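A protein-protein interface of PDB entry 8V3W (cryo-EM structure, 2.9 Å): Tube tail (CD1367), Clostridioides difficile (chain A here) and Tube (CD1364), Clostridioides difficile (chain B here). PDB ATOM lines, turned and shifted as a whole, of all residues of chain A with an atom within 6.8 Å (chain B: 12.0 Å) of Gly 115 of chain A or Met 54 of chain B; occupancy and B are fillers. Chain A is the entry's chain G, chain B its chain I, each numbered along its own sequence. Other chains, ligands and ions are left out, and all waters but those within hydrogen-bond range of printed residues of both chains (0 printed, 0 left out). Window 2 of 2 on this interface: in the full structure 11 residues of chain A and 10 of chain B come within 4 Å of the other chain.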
ATOM      1  N   ARG A 113     -23.813  -3.381 -15.284  1.00  0.00           N
ATOM      2  CA  ARG A 113     -23.932  -3.232 -13.840  1.00  0.00           C
ATOM      3  C   ARG A 113     -24.412  -1.862 -13.373  1.00  0.00           C
ATOM      4  O   ARG A 113     -24.295  -1.566 -12.179  1.00  0.00           O
ATOM      5  CB  ARG A 113     -22.594  -3.540 -13.171  1.00  0.00           C
ATOM      6  CG  ARG A 113     -21.478  -2.634 -13.616  1.00  0.00           C
ATOM      7  CD  ARG A 113     -20.138  -3.139 -13.143  1.00  0.00           C
ATOM      8  NE  ARG A 113     -19.158  -2.064 -13.096  1.00  0.00           N
ATOM      9  CZ  ARG A 113     -17.849  -2.245 -13.015  1.00  0.00           C
ATOM     10  NH1 ARG A 113     -17.322  -3.457 -12.973  1.00  0.00           N
ATOM     11  NH2 ARG A 113     -17.049  -1.184 -12.976  1.00  0.00           N
ATOM     12  N   ASP A 114     -24.937  -1.012 -14.248  1.00  0.00           N
ATOM     13  CA  ASP A 114     -25.471   0.272 -13.806  1.00  0.00           C
ATOM     14  C   ASP A 114     -26.564   0.710 -14.774  1.00  0.00           C
ATOM     15  O   ASP A 114     -27.047  -0.077 -15.591  1.00  0.00           O
ATOM     16  CB  ASP A 114     -24.355   1.314 -13.668  1.00  0.00           C
ATOM     17  CG  ASP A 114     -23.547   1.488 -14.935  1.00  0.00           C
ATOM     18  OD1 ASP A 114     -23.829   0.803 -15.939  1.00  0.00           O
ATOM     19  OD2 ASP A 114     -22.615   2.314 -14.925  1.00  0.00           O
ATOM     20  N   GLY A 115     -26.950   1.978 -14.683  1.00  0.00           N
ATOM     21  CA  GLY A 115     -28.013   2.540 -15.484  1.00  0.00           C
ATOM     22  C   GLY A 115     -27.591   3.205 -16.774  1.00  0.00           C
ATOM     23  O   GLY A 115     -28.398   3.912 -17.382  1.00  0.00           O
ATOM     24  N   THR A 116     -26.359   2.993 -17.224  1.00  0.00           N
ATOM     25  CA  THR A 116     -25.828   3.689 -18.386  1.00  0.00           C
ATOM     26  C   THR A 116     -25.824   2.853 -19.655  1.00  0.00           C
ATOM     27  O   THR A 116     -25.593   3.407 -20.733  1.00  0.00           O
ATOM     28  CB  THR A 116     -24.404   4.165 -18.097  1.00  0.00           C
ATOM     29  OG1 THR A 116     -23.564   3.030 -17.867  1.00  0.00           O
ATOM     30  CG2 THR A 116     -24.383   5.036 -16.872  1.00  0.00           C
ATOM     31  N   ARG A 117     -26.072   1.548 -19.554  1.00  0.00           N
ATOM     32  CA  ARG A 117     -26.033   0.607 -20.675  1.00  0.00           C
ATOM     33  C   ARG A 117     -24.631   0.432 -21.250  1.00  0.00           C
ATOM     34  O   ARG A 117     -24.484   0.032 -22.405  1.00  0.00           O
ATOM     35  CB  ARG A 117     -27.003   1.007 -21.793  1.00  0.00           C
ATOM     36  CG  ARG A 117     -28.435   1.239 -21.351  1.00  0.00           C
ATOM     37  CD  ARG A 117     -29.023   0.019 -20.672  1.00  0.00           C
ATOM     38  NE  ARG A 117     -28.757  -1.216 -21.397  1.00  0.00           N
ATOM     39  CZ  ARG A 117     -29.461  -1.647 -22.433  1.00  0.00           C
ATOM     40  NH1 ARG A 117     -30.488  -0.963 -22.902  1.00  0.00           N
ATOM     41  NH2 ARG A 117     -29.124  -2.795 -23.011  1.00  0.00           N
ATOM     42  N   ASP A 118     -23.592   0.722 -20.473  1.00  0.00           N
ATOM     43  CA  ASP A 118     -22.231   0.393 -20.872  1.00  0.00           C
ATOM     44  C   ASP A 118     -21.922  -1.061 -20.538  1.00  0.00           C
ATOM     45  O   ASP A 118     -22.458  -1.625 -19.583  1.00  0.00           O
ATOM     46  CB  ASP A 118     -21.224   1.306 -20.174  1.00  0.00           C
ATOM     47  CG  ASP A 118     -21.422   2.765 -20.513  1.00  0.00           C
ATOM     48  OD1 ASP A 118     -21.796   3.070 -21.659  1.00  0.00           O
ATOM     49  OD2 ASP A 118     -21.206   3.613 -19.630  1.00  0.00           O
ATOM     50  N   TYR A 120     -19.042  -3.712 -19.566  1.00  0.00           N
ATOM     51  CA  TYR A 120     -17.705  -3.989 -19.063  1.00  0.00           C
ATOM     52  C   TYR A 120     -17.263  -5.387 -19.472  1.00  0.00           C
ATOM     53  O   TYR A 120     -18.058  -6.325 -19.477  1.00  0.00           O
ATOM     54  CB  TYR A 120     -17.671  -3.865 -17.541  1.00  0.00           C
ATOM     55  CG  TYR A 120     -17.937  -2.471 -17.038  1.00  0.00           C
ATOM     56  CD1 TYR A 120     -19.229  -1.975 -16.971  1.00  0.00           C
ATOM     57  CD2 TYR A 120     -16.897  -1.643 -16.651  1.00  0.00           C
ATOM     58  CE1 TYR A 120     -19.476  -0.704 -16.526  1.00  0.00           C
ATOM     59  CE2 TYR A 120     -17.137  -0.369 -16.202  1.00  0.00           C
ATOM     60  CZ  TYR A 120     -18.426   0.096 -16.141  1.00  0.00           C
ATOM     61  OH  TYR A 120     -18.665   1.370 -15.691  1.00  0.00           O
ATOM     62  N   MET B  34     -31.522  16.076  -4.832  1.00  0.00           N
ATOM     63  CA  MET B  34     -31.115  14.921  -5.622  1.00  0.00           C
ATOM     64  C   MET B  34     -29.596  14.809  -5.618  1.00  0.00           C
ATOM     65  O   MET B  34     -28.902  15.795  -5.866  1.00  0.00           O
ATOM     66  CB  MET B  34     -31.618  15.042  -7.059  1.00  0.00           C
ATOM     67  CG  MET B  34     -32.980  14.439  -7.303  1.00  0.00           C
ATOM     68  SD  MET B  34     -32.937  12.645  -7.386  1.00  0.00           S
ATOM     69  CE  MET B  34     -34.622  12.257  -6.952  1.00  0.00           C
ATOM     70  N   GLU B  35     -29.085  13.612  -5.346  1.00  0.00           N
ATOM     71  CA  GLU B  35     -27.652  13.351  -5.327  1.00  0.00           C
ATOM     72  C   GLU B  35     -27.256  12.449  -6.486  1.00  0.00           C
ATOM     73  O   GLU B  35     -27.917  11.446  -6.752  1.00  0.00           O
ATOM     74  CB  GLU B  35     -27.224  12.695  -4.017  1.00  0.00           C
ATOM     75  CG  GLU B  35     -26.763  13.667  -2.968  1.00  0.00           C
ATOM     76  CD  GLU B  35     -27.795  13.882  -1.897  1.00  0.00           C
ATOM     77  OE1 GLU B  35     -28.721  13.054  -1.797  1.00  0.00           O
ATOM     78  OE2 GLU B  35     -27.681  14.878  -1.156  1.00  0.00           O
ATOM     79  N   PHE B  36     -26.160  12.793  -7.152  1.00  0.00           N
ATOM     80  CA  PHE B  36     -25.680  12.058  -8.315  1.00  0.00           C
ATOM     81  C   PHE B  36     -24.441  11.254  -7.953  1.00  0.00           C
ATOM     82  O   PHE B  36     -23.568  11.736  -7.228  1.00  0.00           O
ATOM     83  CB  PHE B  36     -25.361  13.003  -9.469  1.00  0.00           C
ATOM     84  CG  PHE B  36     -26.483  13.925  -9.819  1.00  0.00           C
ATOM     85  CD1 PHE B  36     -27.780  13.459  -9.881  1.00  0.00           C
ATOM     86  CD2 PHE B  36     -26.244  15.261 -10.075  1.00  0.00           C
ATOM     87  CE1 PHE B  36     -28.817  14.306 -10.199  1.00  0.00           C
ATOM     88  CE2 PHE B  36     -27.278  16.110 -10.392  1.00  0.00           C
ATOM     89  CZ  PHE B  36     -28.565  15.632 -10.454  1.00  0.00           C
ATOM     90  N   THR B  37     -24.369  10.029  -8.461  1.00  0.00           N
ATOM     91  CA  THR B  37     -23.250   9.133  -8.206  1.00  0.00           C
ATOM     92  C   THR B  37     -22.304   9.140  -9.398  1.00  0.00           C
ATOM     93  O   THR B  37     -22.745   9.014 -10.544  1.00  0.00           O
ATOM     94  CB  THR B  37     -23.742   7.712  -7.939  1.00  0.00           C
ATOM     95  OG1 THR B  37     -24.993   7.762  -7.247  1.00  0.00           O
ATOM     96  CG2 THR B  37     -22.741   6.953  -7.099  1.00  0.00           C
ATOM     97  N   LYS B  38     -21.012   9.290  -9.127  1.00  0.00           N
ATOM     98  CA  LYS B  38     -19.993   9.368 -10.160  1.00  0.00           C
ATOM     99  C   LYS B  38     -18.989   8.236 -10.007  1.00  0.00           C
ATOM    100  O   LYS B  38     -18.754   7.737  -8.906  1.00  0.00           O
ATOM    101  CB  LYS B  38     -19.249  10.701 -10.112  1.00  0.00           C
ATOM    102  CG  LYS B  38     -20.108  11.912 -10.356  1.00  0.00           C
ATOM    103  CD  LYS B  38     -19.324  13.175 -10.075  1.00  0.00           C
ATOM    104  CE  LYS B  38     -20.024  14.393 -10.623  1.00  0.00           C
ATOM    105  NZ  LYS B  38     -19.291  15.632 -10.275  1.00  0.00           N
ATOM    106  N   GLU B  39     -18.386   7.850 -11.126  1.00  0.00           N
ATOM    107  CA  GLU B  39     -17.312   6.868 -11.153  1.00  0.00           C
ATOM    108  C   GLU B  39     -16.083   7.501 -11.786  1.00  0.00           C
ATOM    109  O   GLU B  39     -16.177   8.090 -12.864  1.00  0.00           O
ATOM    110  CB  GLU B  39     -17.723   5.621 -11.931  1.00  0.00           C
ATOM    111  CG  GLU B  39     -16.583   4.664 -12.173  1.00  0.00           C
ATOM    112  CD  GLU B  39     -16.979   3.494 -13.037  1.00  0.00           C
ATOM    113  OE1 GLU B  39     -17.858   2.716 -12.620  1.00  0.00           O
ATOM    114  OE2 GLU B  39     -16.402   3.346 -14.133  1.00  0.00           O
ATOM    115  N   ASP B  40     -14.938   7.378 -11.118  1.00  0.00           N
ATOM    116  CA  ASP B  40     -13.702   7.958 -11.627  1.00  0.00           C
ATOM    117  C   ASP B  40     -13.145   7.138 -12.782  1.00  0.00           C
ATOM    118  O   ASP B  40     -13.149   5.907 -12.750  1.00  0.00           O
ATOM    119  CB  ASP B  40     -12.661   8.043 -10.515  1.00  0.00           C
ATOM    120  CG  ASP B  40     -12.861   9.244  -9.622  1.00  0.00           C
ATOM    121  OD1 ASP B  40     -13.703  10.098  -9.959  1.00  0.00           O
ATOM    122  OD2 ASP B  40     -12.179   9.336  -8.584  1.00  0.00           O
ATOM    123  N   ILE B  41     -12.650   7.830 -13.803  1.00  0.00           N
ATOM    124  CA  ILE B  41     -12.072   7.198 -14.983  1.00  0.00           C
ATOM    125  C   ILE B  41     -10.600   7.573 -15.049  1.00  0.00           C
ATOM    126  O   ILE B  41     -10.257   8.759 -15.105  1.00  0.00           O
ATOM    127  CB  ILE B  41     -12.804   7.613 -16.269  1.00  0.00           C
ATOM    128  CG1 ILE B  41     -14.308   7.394 -16.113  1.00  0.00           C
ATOM    129  CG2 ILE B  41     -12.268   6.848 -17.458  1.00  0.00           C
ATOM    130  CD1 ILE B  41     -14.704   5.947 -16.048  1.00  0.00           C
ATOM    131  N   ASP B  50     -11.201  11.765 -15.188  1.00  0.00           N
ATOM    132  CA  ASP B  50     -12.540  12.138 -15.623  1.00  0.00           C
ATOM    133  C   ASP B  50     -13.568  11.279 -14.897  1.00  0.00           C
ATOM    134  O   ASP B  50     -13.222  10.379 -14.131  1.00  0.00           O
ATOM    135  CB  ASP B  50     -12.681  11.991 -17.143  1.00  0.00           C
ATOM    136  CG  ASP B  50     -13.571  13.052 -17.752  1.00  0.00           C
ATOM    137  OD1 ASP B  50     -14.435  13.590 -17.035  1.00  0.00           O
ATOM    138  OD2 ASP B  50     -13.396  13.363 -18.947  1.00  0.00           O
ATOM    139  N   THR B  51     -14.850  11.560 -15.142  1.00  0.00           N
ATOM    140  CA  THR B  51     -15.941  10.884 -14.448  1.00  0.00           C
ATOM    141  C   THR B  51     -17.048  10.513 -15.425  1.00  0.00           C
ATOM    142  O   THR B  51     -17.101  10.996 -16.558  1.00  0.00           O
ATOM    143  CB  THR B  51     -16.537  11.748 -13.328  1.00  0.00           C
ATOM    144  OG1 THR B  51     -17.036  12.970 -13.881  1.00  0.00           O
ATOM    145  CG2 THR B  51     -15.503  12.065 -12.265  1.00  0.00           C
ATOM    146  N   LYS B  52     -17.942   9.638 -14.964  1.00  0.00           N
ATOM    147  CA  LYS B  52     -19.195   9.335 -15.643  1.00  0.00           C
ATOM    148  C   LYS B  52     -20.280   9.120 -14.600  1.00  0.00           C
ATOM    149  O   LYS B  52     -20.017   8.572 -13.529  1.00  0.00           O
ATOM    150  CB  LYS B  52     -19.074   8.098 -16.539  1.00  0.00           C
ATOM    151  CG  LYS B  52     -18.617   6.855 -15.808  1.00  0.00           C
ATOM    152  CD  LYS B  52     -18.767   5.609 -16.651  1.00  0.00           C
ATOM    153  CE  LYS B  52     -20.045   4.877 -16.308  1.00  0.00           C
ATOM    154  NZ  LYS B  52     -20.096   3.526 -16.915  1.00  0.00           N
ATOM    155  N   TYR B  53     -21.497   9.560 -14.913  1.00  0.00           N
ATOM    156  CA  TYR B  53     -22.617   9.413 -13.992  1.00  0.00           C
ATOM    157  C   TYR B  53     -23.090   7.964 -13.924  1.00  0.00           C
ATOM    158  O   TYR B  53     -23.187   7.278 -14.941  1.00  0.00           O
ATOM    159  CB  TYR B  53     -23.774  10.307 -14.425  1.00  0.00           C
ATOM    160  CG  TYR B  53     -23.561  11.775 -14.156  1.00  0.00           C
ATOM    161  CD1 TYR B  53     -23.414  12.248 -12.865  1.00  0.00           C
ATOM    162  CD2 TYR B  53     -23.505  12.689 -15.196  1.00  0.00           C
ATOM    163  CE1 TYR B  53     -23.220  13.584 -12.617  1.00  0.00           C
ATOM    164  CE2 TYR B  53     -23.307  14.030 -14.956  1.00  0.00           C
ATOM    165  CZ  TYR B  53     -23.167  14.470 -13.665  1.00  0.00           C
ATOM    166  OH  TYR B  53     -22.976  15.801 -13.412  1.00  0.00           O
ATOM    167  N   MET B  54     -23.405   7.508 -12.713  1.00  0.00           N
ATOM    168  CA  MET B  54     -23.886   6.152 -12.470  1.00  0.00           C
ATOM    169  C   MET B  54     -25.375   6.095 -12.168  1.00  0.00           C
ATOM    170  O   MET B  54     -26.093   5.284 -12.756  1.00  0.00           O
ATOM    171  CB  MET B  54     -23.117   5.520 -11.304  1.00  0.00           C
ATOM    172  CG  MET B  54     -21.922   4.701 -11.700  1.00  0.00           C
ATOM    173  SD  MET B  54     -20.696   4.655 -10.388  1.00  0.00           S
ATOM    174  CE  MET B  54     -21.068   3.076  -9.642  1.00  0.00           C
ATOM    175  N   GLY B  55     -25.849   6.929 -11.255  1.00  0.00           N
ATOM    176  CA  GLY B  55     -27.242   6.920 -10.863  1.00  0.00           C
ATOM    177  C   GLY B  55     -27.562   8.150 -10.047  1.00  0.00           C
ATOM    178  O   GLY B  55     -26.764   9.082  -9.964  1.00  0.00           O
ATOM    179  N   TYR B  56     -28.748   8.150  -9.443  1.00  0.00           N
ATOM    180  CA  TYR B  56     -29.126   9.249  -8.567  1.00  0.00           C
ATOM    181  C   TYR B  56     -30.026   8.745  -7.448  1.00  0.00           C
ATOM    182  O   TYR B  56     -30.608   7.664  -7.529  1.00  0.00           O
ATOM    183  CB  TYR B  56     -29.804  10.389  -9.336  1.00  0.00           C
ATOM    184  CG  TYR B  56     -30.987   9.988 -10.182  1.00  0.00           C
ATOM    185  CD1 TYR B  56     -32.250   9.851  -9.629  1.00  0.00           C
ATOM    186  CD2 TYR B  56     -30.848   9.791 -11.543  1.00  0.00           C
ATOM    187  CE1 TYR B  56     -33.329   9.494 -10.402  1.00  0.00           C
ATOM    188  CE2 TYR B  56     -31.922   9.443 -12.322  1.00  0.00           C
ATOM    189  CZ  TYR B  56     -33.158   9.294 -11.749  1.00  0.00           C
ATOM    190  OH  TYR B  56     -34.229   8.942 -12.532  1.00  0.00           O
ATOM    191  N   LYS B  57     -30.118   9.552  -6.390  1.00  0.00           N
ATOM    192  CA  LYS B  57     -30.935   9.257  -5.223  1.00  0.00           C
ATOM    193  C   LYS B  57     -31.487  10.561  -4.664  1.00  0.00           C
ATOM    194  O   LYS B  57     -30.913  11.629  -4.879  1.00  0.00           O
ATOM    195  CB  LYS B  57     -30.122   8.521  -4.157  1.00  0.00           C
ATOM    196  CG  LYS B  57     -30.957   7.764  -3.154  1.00  0.00           C
ATOM    197  CD  LYS B  57     -30.101   7.193  -2.046  1.00  0.00           C
ATOM    198  CE  LYS B  57     -30.827   6.078  -1.324  1.00  0.00           C
ATOM    199  NZ  LYS B  57     -31.993   6.602  -0.575  1.00  0.00           N
ATOM    200  N   GLY B  58     -32.600  10.472  -3.949  1.00  0.00           N
ATOM    201  CA  GLY B  58     -33.253  11.642  -3.373  1.00  0.00           C
ATOM    202  C   GLY B  58     -33.269  11.599  -1.857  1.00  0.00           C
ATOM    203  O   GLY B  58     -33.473  10.540  -1.265  1.00  0.00           O
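Of the printed residues of chain B, Arg 113 of chain A touches Glu 39.
Of chain B, only Lys 52 (3.4 Å) comes within 4 Å of Asp 114 of chain A.
Of chain B, only Lys 52 and Tyr 53 come within 4 Å of Thr 116 of chain A.
Printed residues of chain B within 4 Å of Tyr 120 of chain A: Glu 39 and Lys 52.
Of chain A, only Gly 115 (3.9 Å) comes within 4 Å of Met 54 of chain B.
The nearest residue of chain B that does not touch Gly 115 of chain A is Gly 55 of chain B (6.1 Å).
The nearest printed residue of chain B that does not touch Arg 113 of chain A is Met 54 of chain B (6.2 Å).
N of Met 54 of chain B is in hydrogen-bond range of O of Thr 37 of chain B, at 2.7 Å.
OG1 of Thr 116 of chain A sits at hydrogen-bond distance from OD2 of Asp 118 of chain A.
O of Lys 52 of chain B sits at hydrogen-bond distance from N of Glu 39 of chain B, 3.0 Å away.
The side-chain hydroxyl (OG1) of Thr 116 of chain A lies within hydrogen-bond range of the side-chain carboxylate (OD1) of Asp 114 of chain A, 3.0 Å away.
Hydrophobic or aromatic side chains of chain A within 4 Å of the printed part of chain B: Tyr 120.
Among the printed residues, 8 pairs touch across the chains.
The side-chain hydroxyl of Tyr 120 of chain A lies within hydrogen-bond range of the side-chain carboxylate of Glu 39 of chain B (3.4 Å).
The side-chain carboxylate of Asp 114 of chain A lies within salt-bridge range of the side-chain amino group of Lys 52 of chain B, 3.4 Å away.
The guanidinium group (NH2) of Arg 113 of chain A lies within salt-bridge range of the side-chain carboxylate (OE1) of Glu 39 of chain B (3.999 Å).
The side-chain hydroxyl (OH) of Tyr 120 of chain A lies within hydrogen-bond range of the side-chain amino group (NZ) of Lys 52 of chain B (2.9 Å).
The side-chain carboxylate (OD2) of Asp 118 of chain A lies within salt-bridge range of the side-chain amino group (NZ) of Lys 52 of chain B (2.9 Å).
Among the printed residues, pairs that only touch across the chains: Thr 116 of chain A with Tyr 53 of chain B, Thr 116 of chain A with Lys 52 of chain B and Gly 115 of chain A with Met 54 of chain B.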
